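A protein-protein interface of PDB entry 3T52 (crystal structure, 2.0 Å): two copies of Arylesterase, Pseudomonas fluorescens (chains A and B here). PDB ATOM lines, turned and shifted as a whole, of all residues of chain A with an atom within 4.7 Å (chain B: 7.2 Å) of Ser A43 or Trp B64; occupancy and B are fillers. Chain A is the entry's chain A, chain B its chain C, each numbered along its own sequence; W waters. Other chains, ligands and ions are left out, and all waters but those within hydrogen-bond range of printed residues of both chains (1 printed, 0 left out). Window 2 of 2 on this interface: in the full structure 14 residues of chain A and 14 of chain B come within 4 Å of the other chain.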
ATOM      1  N   TRP A  16      22.992 -13.761   0.047  1.00  0.00           N
ATOM      2  CA  TRP A  16      23.131 -13.436  -1.374  1.00  0.00           C
ATOM      3  C   TRP A  16      24.542 -13.745  -1.911  1.00  0.00           C
ATOM      4  O   TRP A  16      25.531 -13.470  -1.245  1.00  0.00           O
ATOM      5  CB  TRP A  16      22.869 -11.953  -1.599  1.00  0.00           C
ATOM      6  CG  TRP A  16      21.429 -11.498  -1.509  1.00  0.00           C
ATOM      7  CD1 TRP A  16      20.311 -12.268  -1.308  1.00  0.00           C
ATOM      8  CD2 TRP A  16      20.981 -10.164  -1.635  1.00  0.00           C
ATOM      9  NE1 TRP A  16      19.186 -11.477  -1.303  1.00  0.00           N
ATOM     10  CE2 TRP A  16      19.568 -10.179  -1.505  1.00  0.00           C
ATOM     11  CE3 TRP A  16      21.637  -8.941  -1.851  1.00  0.00           C
ATOM     12  CZ2 TRP A  16      18.793  -9.015  -1.581  1.00  0.00           C
ATOM     13  CZ3 TRP A  16      20.867  -7.765  -1.919  1.00  0.00           C
ATOM     14  CH2 TRP A  16      19.452  -7.819  -1.785  1.00  0.00           C
ATOM     15  N   GLY A  17      24.606 -14.288  -3.129  1.00  0.00           N
ATOM     16  CA  GLY A  17      25.864 -14.420  -3.862  1.00  0.00           C
ATOM     17  C   GLY A  17      26.739 -15.548  -3.353  1.00  0.00           C
ATOM     18  O   GLY A  17      26.319 -16.351  -2.531  1.00  0.00           O
ATOM     19  N   MET A  39      25.203  -4.833   0.186  1.00  0.00           N
ATOM     20  CA  MET A  39      25.066  -6.213  -0.263  1.00  0.00           C
ATOM     21  C   MET A  39      25.093  -6.365  -1.784  1.00  0.00           C
ATOM     22  O   MET A  39      25.766  -7.255  -2.297  1.00  0.00           O
ATOM     23  CB  MET A  39      23.789  -6.860   0.304  1.00  0.00           C
ATOM     24  CG  MET A  39      23.847  -6.970   1.858  1.00  0.00           C
ATOM     25  SD  MET A  39      22.312  -7.673   2.471  1.00  0.00           S
ATOM     26  CE  MET A  39      22.443  -9.359   1.870  1.00  0.00           C
ATOM     27  N   GLU A  40      24.355  -5.518  -2.493  1.00  0.00           N
ATOM     28  CA  GLU A  40      24.390  -5.535  -3.952  1.00  0.00           C
ATOM     29  C   GLU A  40      25.803  -5.237  -4.445  1.00  0.00           C
ATOM     30  O   GLU A  40      26.308  -5.939  -5.299  1.00  0.00           O
ATOM     31  CB  GLU A  40      23.408  -4.534  -4.555  1.00  0.00           C
ATOM     32  CG  GLU A  40      23.255  -4.652  -6.080  1.00  0.00           C
ATOM     33  CD  GLU A  40      24.369  -3.927  -6.872  1.00  0.00           C
ATOM     34  OE1 GLU A  40      24.580  -4.265  -8.060  1.00  0.00           O
ATOM     35  OE2 GLU A  40      25.025  -3.027  -6.316  1.00  0.00           O
ATOM     36  N   TYR A  41      26.427  -4.205  -3.891  1.00  0.00           N
ATOM     37  CA  TYR A  41      27.767  -3.792  -4.305  1.00  0.00           C
ATOM     38  C   TYR A  41      28.800  -4.913  -4.179  1.00  0.00           C
ATOM     39  O   TYR A  41      29.579  -5.165  -5.118  1.00  0.00           O
ATOM     40  CB  TYR A  41      28.187  -2.606  -3.455  1.00  0.00           C
ATOM     41  CG  TYR A  41      29.492  -1.981  -3.871  1.00  0.00           C
ATOM     42  CD1 TYR A  41      29.530  -1.016  -4.878  1.00  0.00           C
ATOM     43  CD2 TYR A  41      30.695  -2.379  -3.279  1.00  0.00           C
ATOM     44  CE1 TYR A  41      30.732  -0.426  -5.260  1.00  0.00           C
ATOM     45  CE2 TYR A  41      31.908  -1.798  -3.659  1.00  0.00           C
ATOM     46  CZ  TYR A  41      31.914  -0.828  -4.661  1.00  0.00           C
ATOM     47  OH  TYR A  41      33.107  -0.246  -5.031  1.00  0.00           O
ATOM     48  N   LEU A  42      28.802  -5.603  -3.038  1.00  0.00           N
ATOM     49  CA  LEU A  42      29.818  -6.619  -2.762  1.00  0.00           C
ATOM     50  C   LEU A  42      29.486  -7.949  -3.403  1.00  0.00           C
ATOM     51  O   LEU A  42      30.387  -8.652  -3.914  1.00  0.00           O
ATOM     52  CB  LEU A  42      30.045  -6.787  -1.254  1.00  0.00           C
ATOM     53  CG  LEU A  42      30.604  -5.547  -0.549  1.00  0.00           C
ATOM     54  CD1 LEU A  42      30.597  -5.784   0.945  1.00  0.00           C
ATOM     55  CD2 LEU A  42      32.049  -5.208  -1.016  1.00  0.00           C
ATOM     56  N   SER A  43      28.207  -8.317  -3.399  1.00  0.00           N
ATOM     57  CA  SER A  43      27.840  -9.558  -4.035  1.00  0.00           C
ATOM     58  C   SER A  43      27.959  -9.520  -5.563  1.00  0.00           C
ATOM     59  O   SER A  43      28.032 -10.557  -6.188  1.00  0.00           O
ATOM     60  CB  SER A  43      26.464 -10.032  -3.598  1.00  0.00           C
ATOM     61  OG  SER A  43      26.535 -10.591  -2.305  1.00  0.00           O
ATOM     62  N   SER A  44      27.949  -8.335  -6.162  1.00  0.00           N
ATOM     63  CA  SER A  44      28.181  -8.178  -7.601  1.00  0.00           C
ATOM     64  C   SER A  44      29.687  -8.233  -7.874  1.00  0.00           C
ATOM     65  O   SER A  44      30.106  -8.248  -9.001  1.00  0.00           O
ATOM     66  CB  SER A  44      27.620  -6.843  -8.103  1.00  0.00           C
ATOM     67  OG  SER A  44      26.211  -6.768  -7.958  1.00  0.00           O
ATOM     68  N   ARG A  45      30.494  -8.232  -6.805  1.00  0.00           N
ATOM     69  CA  ARG A  45      31.965  -8.216  -6.935  1.00  0.00           C
ATOM     70  C   ARG A  45      32.618  -9.414  -6.268  1.00  0.00           C
ATOM     71  O   ARG A  45      33.733  -9.306  -5.738  1.00  0.00           O
ATOM     72  CB  ARG A  45      32.541  -6.915  -6.364  1.00  0.00           C
ATOM     73  CG  ARG A  45      32.265  -5.697  -7.224  1.00  0.00           C
ATOM     74  CD  ARG A  45      32.553  -4.404  -6.490  1.00  0.00           C
ATOM     75  NE  ARG A  45      32.276  -3.246  -7.343  1.00  0.00           N
ATOM     76  CZ  ARG A  45      31.066  -2.831  -7.717  1.00  0.00           C
ATOM     77  NH1 ARG A  45      29.949  -3.437  -7.312  1.00  0.00           N
ATOM     78  NH2 ARG A  45      30.964  -1.779  -8.496  1.00  0.00           N
ATOM     79  N   GLY A  46      31.918 -10.543  -6.283  1.00  0.00           N
ATOM     80  CA  GLY A  46      32.477 -11.825  -5.867  1.00  0.00           C
ATOM     81  C   GLY A  46      32.391 -12.210  -4.394  1.00  0.00           C
ATOM     82  O   GLY A  46      33.052 -13.167  -3.968  1.00  0.00           O
ATOM     83  N   TYR A  47      31.602 -11.477  -3.603  1.00  0.00           N
ATOM     84  CA  TYR A  47      31.416 -11.821  -2.187  1.00  0.00           C
ATOM     85  C   TYR A  47      30.025 -12.377  -1.896  1.00  0.00           C
ATOM     86  O   TYR A  47      29.044 -12.044  -2.599  1.00  0.00           O
ATOM     87  CB  TYR A  47      31.689 -10.591  -1.314  1.00  0.00           C
ATOM     88  CG  TYR A  47      33.145 -10.191  -1.359  1.00  0.00           C
ATOM     89  CD1 TYR A  47      34.079 -10.798  -0.502  1.00  0.00           C
ATOM     90  CD2 TYR A  47      33.609  -9.248  -2.277  1.00  0.00           C
ATOM     91  CE1 TYR A  47      35.443 -10.459  -0.552  1.00  0.00           C
ATOM     92  CE2 TYR A  47      34.973  -8.894  -2.328  1.00  0.00           C
ATOM     93  CZ  TYR A  47      35.870  -9.512  -1.466  1.00  0.00           C
ATOM     94  OH  TYR A  47      37.195  -9.179  -1.504  1.00  0.00           O
ATOM     95  N   ARG A  48      29.948 -13.223  -0.869  1.00  0.00           N
ATOM     96  CA  ARG A  48      28.676 -13.695  -0.330  1.00  0.00           C
ATOM     97  C   ARG A  48      28.244 -12.744   0.781  1.00  0.00           C
ATOM     98  O   ARG A  48      29.013 -12.493   1.699  1.00  0.00           O
ATOM     99  CB  ARG A  48      28.823 -15.115   0.225  1.00  0.00           C
ATOM    100  CG  ARG A  48      27.521 -15.714   0.776  1.00  0.00           C
ATOM    101  CD  ARG A  48      27.790 -17.134   1.196  1.00  0.00           C
ATOM    102  NE  ARG A  48      26.640 -17.799   1.789  1.00  0.00           N
ATOM    103  CZ  ARG A  48      26.733 -18.951   2.447  1.00  0.00           C
ATOM    104  NH1 ARG A  48      27.929 -19.532   2.588  1.00  0.00           N
ATOM    105  NH2 ARG A  48      25.656 -19.523   2.956  1.00  0.00           N
ATOM    106  N   THR A  49      27.030 -12.190   0.688  1.00  0.00           N
ATOM    107  CA  THR A  49      26.558 -11.233   1.697  1.00  0.00           C
ATOM    108  C   THR A  49      25.334 -11.796   2.441  1.00  0.00           C
ATOM    109  O   THR A  49      24.420 -12.393   1.833  1.00  0.00           O
ATOM    110  CB  THR A  49      26.281  -9.790   1.111  1.00  0.00           C
ATOM    111  OG1 THR A  49      25.308  -9.863   0.060  1.00  0.00           O
ATOM    112  CG2 THR A  49      27.546  -9.125   0.634  1.00  0.00           C
ATOM    113  N   THR B   9      13.433 -20.972  -3.380  1.00  0.00           N
ATOM    114  CA  THR B   9      12.759 -19.679  -3.196  1.00  0.00           C
ATOM    115  C   THR B   9      11.287 -19.853  -2.778  1.00  0.00           C
ATOM    116  O   THR B   9      10.487 -20.462  -3.486  1.00  0.00           O
ATOM    117  CB  THR B   9      12.848 -18.819  -4.491  1.00  0.00           C
ATOM    118  OG1 THR B   9      14.222 -18.520  -4.783  1.00  0.00           O
ATOM    119  CG2 THR B   9      12.061 -17.500  -4.339  1.00  0.00           C
ATOM    120  N   ARG B  55       9.110 -13.585  -7.353  1.00  0.00           N
ATOM    121  CA  ARG B  55      10.338 -13.664  -6.547  1.00  0.00           C
ATOM    122  C   ARG B  55      11.022 -12.305  -6.471  1.00  0.00           C
ATOM    123  O   ARG B  55      11.162 -11.609  -7.482  1.00  0.00           O
ATOM    124  CB  ARG B  55      11.352 -14.706  -7.096  1.00  0.00           C
ATOM    125  CG  ARG B  55      11.790 -14.508  -8.570  1.00  0.00           C
ATOM    126  CD  ARG B  55      12.969 -15.493  -8.897  1.00  0.00           C
ATOM    127  NE  ARG B  55      12.553 -16.903  -8.798  1.00  0.00           N
ATOM    128  CZ  ARG B  55      13.367 -17.899  -8.422  1.00  0.00           C
ATOM    129  NH1 ARG B  55      12.911 -19.153  -8.377  1.00  0.00           N
ATOM    130  NH2 ARG B  55      14.634 -17.657  -8.102  1.00  0.00           N
ATOM    131  N   GLN B  62      13.607 -13.212  -1.443  1.00  0.00           N
ATOM    132  CA  GLN B  62      14.400 -12.348  -2.305  1.00  0.00           C
ATOM    133  C   GLN B  62      15.736 -13.023  -2.716  1.00  0.00           C
ATOM    134  O   GLN B  62      16.803 -12.663  -2.211  1.00  0.00           O
ATOM    135  CB  GLN B  62      14.700 -11.030  -1.590  1.00  0.00           C
ATOM    136  CG  GLN B  62      13.430 -10.295  -1.070  1.00  0.00           C
ATOM    137  CD  GLN B  62      13.782  -8.996  -0.343  1.00  0.00           C
ATOM    138  OE1 GLN B  62      14.968  -8.667  -0.171  1.00  0.00           O
ATOM    139  NE2 GLN B  62      12.761  -8.236   0.059  1.00  0.00           N
ATOM    140  N   PRO B  63      15.669 -13.998  -3.641  1.00  0.00           N
ATOM    141  CA  PRO B  63      16.917 -14.690  -4.035  1.00  0.00           C
ATOM    142  C   PRO B  63      17.853 -13.806  -4.856  1.00  0.00           C
ATOM    143  O   PRO B  63      17.389 -12.965  -5.665  1.00  0.00           O
ATOM    144  CB  PRO B  63      16.410 -15.871  -4.887  1.00  0.00           C
ATOM    145  CG  PRO B  63      15.101 -15.346  -5.496  1.00  0.00           C
ATOM    146  CD  PRO B  63      14.481 -14.618  -4.264  1.00  0.00           C
ATOM    147  N   TRP B  64      19.162 -14.010  -4.654  1.00  0.00           N
ATOM    148  CA  TRP B  64      20.202 -13.320  -5.424  1.00  0.00           C
ATOM    149  C   TRP B  64      20.129 -13.757  -6.887  1.00  0.00           C
ATOM    150  O   TRP B  64      20.320 -12.935  -7.788  1.00  0.00           O
ATOM    151  CB  TRP B  64      21.611 -13.605  -4.877  1.00  0.00           C
ATOM    152  CG  TRP B  64      22.731 -12.907  -5.681  1.00  0.00           C
ATOM    153  CD1 TRP B  64      23.604 -13.489  -6.592  1.00  0.00           C
ATOM    154  CD2 TRP B  64      23.063 -11.512  -5.649  1.00  0.00           C
ATOM    155  NE1 TRP B  64      24.454 -12.528  -7.115  1.00  0.00           N
ATOM    156  CE2 TRP B  64      24.142 -11.310  -6.556  1.00  0.00           C
ATOM    157  CE3 TRP B  64      22.544 -10.408  -4.951  1.00  0.00           C
ATOM    158  CZ2 TRP B  64      24.722 -10.048  -6.769  1.00  0.00           C
ATOM    159  CZ3 TRP B  64      23.126  -9.140  -5.161  1.00  0.00           C
ATOM    160  CH2 TRP B  64      24.210  -8.981  -6.070  1.00  0.00           C
ATOM    161  N   THR B  65      19.827 -15.033  -7.120  1.00  0.00           N
ATOM    162  CA  THR B  65      19.840 -15.560  -8.500  1.00  0.00           C
ATOM    163  C   THR B  65      18.443 -15.855  -8.999  1.00  0.00           C
ATOM    164  O   THR B  65      17.487 -15.960  -8.220  1.00  0.00           O
ATOM    165  CB  THR B  65      20.659 -16.890  -8.623  1.00  0.00           C
ATOM    166  OG1 THR B  65      19.996 -17.893  -7.864  1.00  0.00           O
ATOM    167  CG2 THR B  65      22.108 -16.733  -8.111  1.00  0.00           C
ATOM    168  N   GLY B  66      18.338 -16.016 -10.314  1.00  0.00           N
ATOM    169  CA  GLY B  66      17.099 -16.451 -10.931  1.00  0.00           C
ATOM    170  C   GLY B  66      16.153 -15.302 -11.217  1.00  0.00           C
ATOM    171  O   GLY B  66      14.974 -15.527 -11.445  1.00  0.00           O
ATOM    172  N   ASN B  67      16.658 -14.068 -11.211  1.00  0.00           N
ATOM    173  CA  ASN B  67      15.807 -12.897 -11.526  1.00  0.00           C
ATOM    174  C   ASN B  67      15.801 -12.635 -13.038  1.00  0.00           C
ATOM    175  O   ASN B  67      16.391 -11.665 -13.507  1.00  0.00           O
ATOM    176  CB  ASN B  67      16.245 -11.644 -10.728  1.00  0.00           C
ATOM    177  CG  ASN B  67      16.164 -11.858  -9.205  1.00  0.00           C
ATOM    178  OD1 ASN B  67      15.096 -12.134  -8.655  1.00  0.00           O
ATOM    179  ND2 ASN B  67      17.302 -11.764  -8.536  1.00  0.00           N
ATOM    180  N   SER B 187      13.090  -6.530  -2.999  1.00  0.00           N
ATOM    181  CA  SER B 187      14.534  -6.550  -3.026  1.00  0.00           C
ATOM    182  C   SER B 187      15.082  -5.478  -3.980  1.00  0.00           C
ATOM    183  O   SER B 187      14.571  -5.287  -5.096  1.00  0.00           O
ATOM    184  CB  SER B 187      14.984  -7.936  -3.523  1.00  0.00           C
ATOM    185  OG  SER B 187      16.347  -7.937  -3.928  1.00  0.00           O
ATOM    186  N   LYS B 189      17.950  -5.828  -5.315  1.00  0.00           N
ATOM    187  CA  LYS B 189      18.547  -6.695  -6.333  1.00  0.00           C
ATOM    188  C   LYS B 189      17.485  -7.114  -7.365  1.00  0.00           C
ATOM    189  O   LYS B 189      17.716  -7.007  -8.576  1.00  0.00           O
ATOM    190  CB  LYS B 189      19.257  -7.898  -5.692  1.00  0.00           C
ATOM    191  CG  LYS B 189      19.648  -9.036  -6.667  1.00  0.00           C
ATOM    192  CD  LYS B 189      20.706  -8.568  -7.684  1.00  0.00           C
ATOM    193  CE  LYS B 189      21.323  -9.746  -8.429  1.00  0.00           C
ATOM    194  NZ  LYS B 189      22.171  -9.181  -9.504  1.00  0.00           N
ATOM    195  N   ALA B 190      16.338  -7.593  -6.899  1.00  0.00           N
ATOM    196  CA  ALA B 190      15.312  -8.000  -7.856  1.00  0.00           C
ATOM    197  C   ALA B 190      14.798  -6.804  -8.645  1.00  0.00           C
ATOM    198  O   ALA B 190      14.551  -6.912  -9.837  1.00  0.00           O
ATOM    199  CB  ALA B 190      14.171  -8.696  -7.169  1.00  0.00           C
ATOM    200  N   ASP B 193      17.524  -6.085 -11.301  1.00  0.00           N
ATOM    201  CA  ASP B 193      17.584  -7.220 -12.259  1.00  0.00           C
ATOM    202  C   ASP B 193      16.374  -7.272 -13.173  1.00  0.00           C
ATOM    203  O   ASP B 193      16.502  -7.662 -14.332  1.00  0.00           O
ATOM    204  CB  ASP B 193      17.671  -8.586 -11.556  1.00  0.00           C
ATOM    205  CG  ASP B 193      19.100  -8.996 -11.187  1.00  0.00           C
ATOM    206  OD1 ASP B 193      20.053  -8.239 -11.454  1.00  0.00           O
ATOM    207  OD2 ASP B 193      19.250 -10.083 -10.585  1.00  0.00           O
HETATM  208  O   HOH W   1      23.732  -7.072  -9.558  1.00  0.00           O
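The side-chain hydroxyl (OG) of Ser A43 lies within hydrogen-bond range of the backbone carbonyl oxygen (O) of Trp A16.
The backbone carbonyl oxygen of Met A39 sits close to the side-chain hydroxyl of Ser A43.
The backbone carbonyl oxygen of Glu A40 is in hydrogen-bond range of the side-chain hydroxyl of Ser A44 (2.8 Å).
The side-chain hydroxyl of Ser A43 sits at hydrogen-bond distance from the backbone carbonyl oxygen of Tyr A47 (2.9 Å).
O of Trp B64 sits at hydrogen-bond distance from ND2 of Asn B67.
NZ of Lys B189 is in salt-bridge range of OD1 of Asp B193, 3.0 Å away.
No position is printed for both chains.
Printed residues of chain A that touch a printed residue of chain B: Trp A16, Gly A17, Glu A40, Ser A43 and Ser A44.
Hydrophobic or aromatic side chains of chain A within 4 Å of the printed part of chain B: Trp A16.
Of the 12 printed residues of chain B, 4 touch a printed residue of chain A.
Hydrophobic or aromatic side chains of chain B within 4 Å of the printed part of chain A: Trp B64.
Among the printed residues, 8 pairs touch across the chains.
Water W1 lies within hydrogen-bond range of the side-chain amino group of Lys B189 (2.6 Å), the side-chain hydroxyl of Ser A44 (3.0 Å) and the side-chain carboxylate of Glu A40 (3.3 Å).
Ser A43 touches just one residue of chain B: Trp B64.
Printed residues of chain A within 4 Å of Trp B64: Trp A16 (3.5 Å), Gly A17 (3.5 Å), Glu A40 (3.8 Å), Ser A43 (3.4 Å) and Ser A44 (3.5 Å).
Printed residues of chain B within 4 Å of Glu A40: Trp B64 (3.8 Å).
Of the printed residues of chain B, Trp A16 touches Gln B62, Trp B64, Ser B187 and Lys B189.
Of the printed residues of chain B, Gly A17 touches Trp B64.
Of the printed residues of chain A, Gln B62 touches Trp A16.
The nearest printed residue of chain A that does not touch Ser B187 is Glu A40 (7.9 Å).
The indole nitrogen (NE1) of Trp A16 sits at hydrogen-bond distance from the backbone carbonyl oxygen (O) of Gln B62 (2.8 Å).
Trp A16 touches Trp B64 (CE3 to CE3, 3.5 Å).
Ser B187 touches Trp A16.
Trp A16 touches Lys B189.
Trp B64 touches Gly A17 (CG to N, 3.5 Å).
Glu A40 touches Trp B64 (O to CH2, 3.8 Å).
CZ2 of Trp B64 touches O of Ser A43 (3.4 Å).
Ser A44 touches Trp B64 (OG to CH2, 3.5 Å).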
